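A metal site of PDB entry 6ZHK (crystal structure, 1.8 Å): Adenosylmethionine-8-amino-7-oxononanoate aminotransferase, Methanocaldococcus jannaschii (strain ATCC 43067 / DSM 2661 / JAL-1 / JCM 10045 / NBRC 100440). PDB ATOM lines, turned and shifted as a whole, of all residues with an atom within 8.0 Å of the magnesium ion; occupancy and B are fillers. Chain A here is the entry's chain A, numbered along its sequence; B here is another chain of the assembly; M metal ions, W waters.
Within 4 Å of the magnesium ion: Val 106, Thr 109, Pro 110 and Leu 113.
The magnesium ion is bound by water W1, the backbone carbonyl oxygen (O) of Leu 113, the backbone carbonyl oxygen (O) of Val 106, the backbone carbonyl oxygen (O) of Pro 110 and the side-chain hydroxyl (OG1) of Thr 109. The magnesium ion has five donor atoms within binding distance. Slightly farther from the magnesium ion lies the backbone carbonyl oxygen (O) of Thr 109 (2.7 Å).
O of Leu 105 sits close to OG1 of Thr 109 (2.8 Å). O of Thr 109 sits at hydrogen-bond distance from NZ of Lys 111, at 2.9 Å.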
ATOM      1  N   ALA A 102      17.452 -14.570 -23.027  1.00  0.00           N
ATOM      2  CA  ALA A 102      18.698 -13.821 -22.734  1.00  0.00           C
ATOM      3  C   ALA A 102      19.156 -13.160 -24.037  1.00  0.00           C
ATOM      4  O   ALA A 102      19.598 -12.031 -24.055  1.00  0.00           O
ATOM      5  CB  ALA A 102      19.793 -14.715 -22.145  1.00  0.00           C
ATOM      6  N   LYS A 103      19.048 -13.890 -25.158  1.00  0.00           N
ATOM      7  CA  LYS A 103      19.436 -13.293 -26.430  1.00  0.00           C
ATOM      8  C   LYS A 103      18.535 -12.084 -26.736  1.00  0.00           C
ATOM      9  O   LYS A 103      19.007 -11.048 -27.204  1.00  0.00           O
ATOM     10  CB  LYS A 103      19.363 -14.344 -27.530  1.00  0.00           C
ATOM     11  CG  LYS A 103      19.609 -13.777 -28.945  1.00  0.00           C
ATOM     12  CD  LYS A 103      19.888 -14.907 -29.955  1.00  0.00           C
ATOM     13  CE  LYS A 103      19.909 -14.443 -31.403  1.00  0.00           C
ATOM     14  NZ  LYS A 103      20.538 -13.115 -31.541  1.00  0.00           N
ATOM     15  N   LYS A 104      17.229 -12.189 -26.506  1.00  0.00           N
ATOM     16  CA  LYS A 104      16.370 -11.053 -26.811  1.00  0.00           C
ATOM     17  C   LYS A 104      16.735  -9.839 -25.960  1.00  0.00           C
ATOM     18  O   LYS A 104      16.720  -8.705 -26.438  1.00  0.00           O
ATOM     19  CB  LYS A 104      14.899 -11.378 -26.548  1.00  0.00           C
ATOM     20  CG  LYS A 104      14.225 -12.389 -27.470  1.00  0.00           C
ATOM     21  CD  LYS A 104      14.187 -12.041 -28.949  1.00  0.00           C
ATOM     22  CE  LYS A 104      13.097 -12.844 -29.667  1.00  0.00           C
ATOM     23  NZ  LYS A 104      13.443 -12.971 -31.104  1.00  0.00           N
ATOM     24  N   LEU A 105      16.999 -10.053 -24.661  1.00  0.00           N
ATOM     25  CA  LEU A 105      17.339  -8.964 -23.743  1.00  0.00           C
ATOM     26  C   LEU A 105      18.648  -8.282 -24.155  1.00  0.00           C
ATOM     27  O   LEU A 105      18.692  -7.064 -24.129  1.00  0.00           O
ATOM     28  CB  LEU A 105      17.444  -9.493 -22.296  1.00  0.00           C
ATOM     29  CG  LEU A 105      16.094  -9.791 -21.666  1.00  0.00           C
ATOM     30  CD1 LEU A 105      16.257 -10.519 -20.332  1.00  0.00           C
ATOM     31  CD2 LEU A 105      15.213  -8.562 -21.518  1.00  0.00           C
ATOM     32  N   VAL A 106      19.674  -9.057 -24.561  1.00  0.00           N
ATOM     33  CA  VAL A 106      20.942  -8.479 -24.987  1.00  0.00           C
ATOM     34  C   VAL A 106      20.688  -7.630 -26.240  1.00  0.00           C
ATOM     35  O   VAL A 106      21.223  -6.496 -26.324  1.00  0.00           O
ATOM     36  CB  VAL A 106      22.001  -9.604 -25.159  1.00  0.00           C
ATOM     37  CG1 VAL A 106      23.246  -9.156 -25.939  1.00  0.00           C
ATOM     38  CG2 VAL A 106      22.440 -10.184 -23.765  1.00  0.00           C
ATOM     39  N   ASP A 107      19.886  -8.214 -27.167  1.00  0.00           N
ATOM     40  CA  ASP A 107      19.615  -7.562 -28.456  1.00  0.00           C
ATOM     41  C   ASP A 107      18.810  -6.271 -28.284  1.00  0.00           C
ATOM     42  O   ASP A 107      19.009  -5.360 -29.068  1.00  0.00           O
ATOM     43  CB  ASP A 107      18.942  -8.512 -29.462  1.00  0.00           C
ATOM     44  CG  ASP A 107      19.888  -9.577 -29.985  1.00  0.00           C
ATOM     45  OD1 ASP A 107      21.164  -9.443 -29.761  1.00  0.00           O
ATOM     46  OD2 ASP A 107      19.376 -10.568 -30.543  1.00  0.00           O
ATOM     47  N   ILE A 108      17.874  -6.187 -27.341  1.00  0.00           N
ATOM     48  CA  ILE A 108      17.107  -4.943 -27.255  1.00  0.00           C
ATOM     49  C   ILE A 108      17.754  -3.896 -26.369  1.00  0.00           C
ATOM     50  O   ILE A 108      17.249  -2.788 -26.310  1.00  0.00           O
ATOM     51  CB  ILE A 108      15.667  -5.137 -26.778  1.00  0.00           C
ATOM     52  CG1 ILE A 108      15.660  -5.832 -25.419  1.00  0.00           C
ATOM     53  CG2 ILE A 108      14.812  -5.830 -27.832  1.00  0.00           C
ATOM     54  CD1 ILE A 108      14.260  -5.901 -24.873  1.00  0.00           C
ATOM     55  N   THR A 109      18.791  -4.259 -25.614  1.00  0.00           N
ATOM     56  CA  THR A 109      19.382  -3.228 -24.762  1.00  0.00           C
ATOM     57  C   THR A 109      20.584  -2.648 -25.472  1.00  0.00           C
ATOM     58  O   THR A 109      21.101  -3.259 -26.409  1.00  0.00           O
ATOM     59  CB  THR A 109      19.859  -3.839 -23.442  1.00  0.00           C
ATOM     60  OG1 THR A 109      20.551  -5.062 -23.736  1.00  0.00           O
ATOM     61  CG2 THR A 109      18.673  -4.199 -22.573  1.00  0.00           C
ATOM     62  N   PRO A 110      21.129  -1.500 -24.994  1.00  0.00           N
ATOM     63  CA  PRO A 110      22.380  -0.977 -25.533  1.00  0.00           C
ATOM     64  C   PRO A 110      23.431  -2.056 -25.804  1.00  0.00           C
ATOM     65  O   PRO A 110      23.500  -3.134 -25.159  1.00  0.00           O
ATOM     66  CB  PRO A 110      22.824   0.094 -24.511  1.00  0.00           C
ATOM     67  CG  PRO A 110      21.463   0.603 -23.975  1.00  0.00           C
ATOM     68  CD  PRO A 110      20.584  -0.656 -23.920  1.00  0.00           C
ATOM     69  N   LYS A 111      24.230  -1.716 -26.836  1.00  0.00           N
ATOM     70  CA  LYS A 111      25.094  -2.723 -27.413  1.00  0.00           C
ATOM     71  C   LYS A 111      26.223  -3.122 -26.480  1.00  0.00           C
ATOM     72  O   LYS A 111      26.768  -4.186 -26.699  1.00  0.00           O
ATOM     73  CB  LYS A 111      25.631  -2.317 -28.783  1.00  0.00           C
ATOM     74  CG  LYS A 111      24.734  -2.811 -29.928  1.00  0.00           C
ATOM     75  CD  LYS A 111      23.375  -2.134 -29.984  1.00  0.00           C
ATOM     76  CE  LYS A 111      22.190  -3.057 -29.757  1.00  0.00           C
ATOM     77  NZ  LYS A 111      20.996  -2.393 -29.145  1.00  0.00           N
ATOM     78  N   HIS A 112      26.592  -2.289 -25.495  1.00  0.00           N
ATOM     79  CA  HIS A 112      27.689  -2.668 -24.625  1.00  0.00           C
ATOM     80  C   HIS A 112      27.178  -3.623 -23.537  1.00  0.00           C
ATOM     81  O   HIS A 112      27.996  -4.144 -22.789  1.00  0.00           O
ATOM     82  CB  HIS A 112      28.374  -1.476 -23.955  1.00  0.00           C
ATOM     83  CG  HIS A 112      27.445  -0.655 -23.125  1.00  0.00           C
ATOM     84  ND1 HIS A 112      26.502   0.164 -23.698  1.00  0.00           N
ATOM     85  CD2 HIS A 112      27.290  -0.546 -21.784  1.00  0.00           C
ATOM     86  CE1 HIS A 112      25.776   0.734 -22.742  1.00  0.00           C
ATOM     87  NE2 HIS A 112      26.246   0.323 -21.563  1.00  0.00           N
ATOM     88  N   LEU A 113      25.864  -3.821 -23.471  1.00  0.00           N
ATOM     89  CA  LEU A 113      25.333  -4.736 -22.439  1.00  0.00           C
ATOM     90  C   LEU A 113      25.000  -6.056 -23.121  1.00  0.00           C
ATOM     91  O   LEU A 113      24.051  -6.165 -23.933  1.00  0.00           O
ATOM     92  CB  LEU A 113      24.100  -4.128 -21.753  1.00  0.00           C
ATOM     93  CG  LEU A 113      24.305  -2.782 -21.049  1.00  0.00           C
ATOM     94  CD1 LEU A 113      22.990  -2.098 -20.665  1.00  0.00           C
ATOM     95  CD2 LEU A 113      25.149  -2.949 -19.779  1.00  0.00           C
ATOM     96  N   THR A 114      25.813  -7.066 -22.740  1.00  0.00           N
ATOM     97  CA  THR A 114      25.982  -8.276 -23.513  1.00  0.00           C
ATOM     98  C   THR A 114      25.789  -9.525 -22.653  1.00  0.00           C
ATOM     99  O   THR A 114      25.908 -10.641 -23.166  1.00  0.00           O
ATOM    100  CB  THR A 114      27.399  -8.316 -24.095  1.00  0.00           C
ATOM    101  OG1 THR A 114      28.307  -8.002 -23.042  1.00  0.00           O
ATOM    102  CG2 THR A 114      27.599  -7.303 -25.208  1.00  0.00           C
ATOM    103  N   LYS A 115      25.578  -9.368 -21.350  1.00  0.00           N
ATOM    104  CA  LYS A 115      25.472 -10.571 -20.513  1.00  0.00           C
ATOM    105  C   LYS A 115      24.268 -10.406 -19.586  1.00  0.00           C
ATOM    106  O   LYS A 115      23.951  -9.275 -19.216  1.00  0.00           O
ATOM    107  CB  LYS A 115      26.726 -10.725 -19.650  1.00  0.00           C
ATOM    108  CG  LYS A 115      27.990 -11.074 -20.469  1.00  0.00           C
ATOM    109  CD  LYS A 115      27.884 -12.447 -21.091  1.00  0.00           C
ATOM    110  CE  LYS A 115      29.133 -12.892 -21.831  1.00  0.00           C
ATOM    111  NZ  LYS A 115      29.113 -12.384 -23.223  1.00  0.00           N
ATOM    112  N   VAL A 116      23.624 -11.527 -19.221  1.00  0.00           N
ATOM    113  CA  VAL A 116      22.358 -11.488 -18.503  1.00  0.00           C
ATOM    114  C   VAL A 116      22.478 -12.421 -17.299  1.00  0.00           C
ATOM    115  O   VAL A 116      22.814 -13.591 -17.495  1.00  0.00           O
ATOM    116  CB  VAL A 116      21.172 -11.972 -19.398  1.00  0.00           C
ATOM    117  CG1 VAL A 116      19.910 -12.209 -18.571  1.00  0.00           C
ATOM    118  CG2 VAL A 116      20.893 -10.952 -20.480  1.00  0.00           C
ATOM    119  N   PHE A 281      13.992   1.874 -22.737  1.00  0.00           N
ATOM    120  CA  PHE A 281      14.809   1.985 -21.530  1.00  0.00           C
ATOM    121  C   PHE A 281      15.322   3.401 -21.477  1.00  0.00           C
ATOM    122  O   PHE A 281      15.588   3.989 -22.542  1.00  0.00           O
ATOM    123  CB  PHE A 281      16.035   1.061 -21.605  1.00  0.00           C
ATOM    124  CG  PHE A 281      15.668  -0.380 -21.816  1.00  0.00           C
ATOM    125  CD1 PHE A 281      15.142  -1.118 -20.755  1.00  0.00           C
ATOM    126  CD2 PHE A 281      15.811  -0.981 -23.059  1.00  0.00           C
ATOM    127  CE1 PHE A 281      14.761  -2.434 -20.969  1.00  0.00           C
ATOM    128  CE2 PHE A 281      15.460  -2.316 -23.277  1.00  0.00           C
ATOM    129  CZ  PHE A 281      14.905  -3.043 -22.217  1.00  0.00           C
ATOM    130  N   LEU A 297      22.988  -2.680 -15.747  1.00  0.00           N
ATOM    131  CA  LEU A 297      21.590  -2.285 -15.911  1.00  0.00           C
ATOM    132  C   LEU A 297      20.748  -3.302 -15.127  1.00  0.00           C
ATOM    133  O   LEU A 297      20.839  -4.487 -15.427  1.00  0.00           O
ATOM    134  CB  LEU A 297      21.217  -2.337 -17.399  1.00  0.00           C
ATOM    135  CG  LEU A 297      19.717  -2.075 -17.714  1.00  0.00           C
ATOM    136  CD1 LEU A 297      19.363  -0.651 -17.257  1.00  0.00           C
ATOM    137  CD2 LEU A 297      19.425  -2.307 -19.201  1.00  0.00           C
ATOM    138  N   LEU A 314      22.007  -6.871 -16.223  1.00  0.00           N
ATOM    139  CA  LEU A 314      22.804  -6.995 -17.433  1.00  0.00           C
ATOM    140  C   LEU A 314      24.139  -6.245 -17.235  1.00  0.00           C
ATOM    141  O   LEU A 314      24.157  -5.160 -16.666  1.00  0.00           O
ATOM    142  CB  LEU A 314      22.002  -6.334 -18.579  1.00  0.00           C
ATOM    143  CG  LEU A 314      21.105  -7.304 -19.321  1.00  0.00           C
ATOM    144  CD1 LEU A 314      19.917  -7.789 -18.468  1.00  0.00           C
ATOM    145  CD2 LEU A 314      20.750  -6.812 -20.722  1.00  0.00           C
ATOM    146  N   THR A 315      25.233  -6.796 -17.774  1.00  0.00           N
ATOM    147  CA  THR A 315      26.559  -6.202 -17.617  1.00  0.00           C
ATOM    148  C   THR A 315      27.320  -6.243 -18.962  1.00  0.00           C
ATOM    149  O   THR A 315      26.870  -6.880 -19.936  1.00  0.00           O
ATOM    150  CB  THR A 315      27.421  -6.906 -16.559  1.00  0.00           C
ATOM    151  OG1 THR A 315      27.898  -8.120 -17.125  1.00  0.00           O
ATOM    152  CG2 THR A 315      26.647  -7.349 -15.332  1.00  0.00           C
ATOM    153  N   TYR B  20      25.332 -15.558 -23.832  1.00  0.00           N
ATOM    154  CA  TYR B  20      24.453 -14.510 -23.296  1.00  0.00           C
ATOM    155  C   TYR B  20      24.138 -14.664 -21.809  1.00  0.00           C
ATOM    156  O   TYR B  20      23.747 -13.688 -21.178  1.00  0.00           O
ATOM    157  CB  TYR B  20      23.132 -14.482 -24.057  1.00  0.00           C
ATOM    158  CG  TYR B  20      23.327 -14.120 -25.501  1.00  0.00           C
ATOM    159  CD1 TYR B  20      23.807 -12.868 -25.857  1.00  0.00           C
ATOM    160  CD2 TYR B  20      23.000 -15.023 -26.522  1.00  0.00           C
ATOM    161  CE1 TYR B  20      23.973 -12.509 -27.197  1.00  0.00           C
ATOM    162  CE2 TYR B  20      23.154 -14.684 -27.869  1.00  0.00           C
ATOM    163  CZ  TYR B  20      23.656 -13.432 -28.190  1.00  0.00           C
ATOM    164  OH  TYR B  20      23.842 -13.102 -29.504  1.00  0.00           O
HETATM  165 MG    MG M   1      22.614  -5.157 -25.260  1.00  0.00          MG
HETATM  166  O   HOH W   1      23.826  -5.792 -26.887  1.00  0.00           O
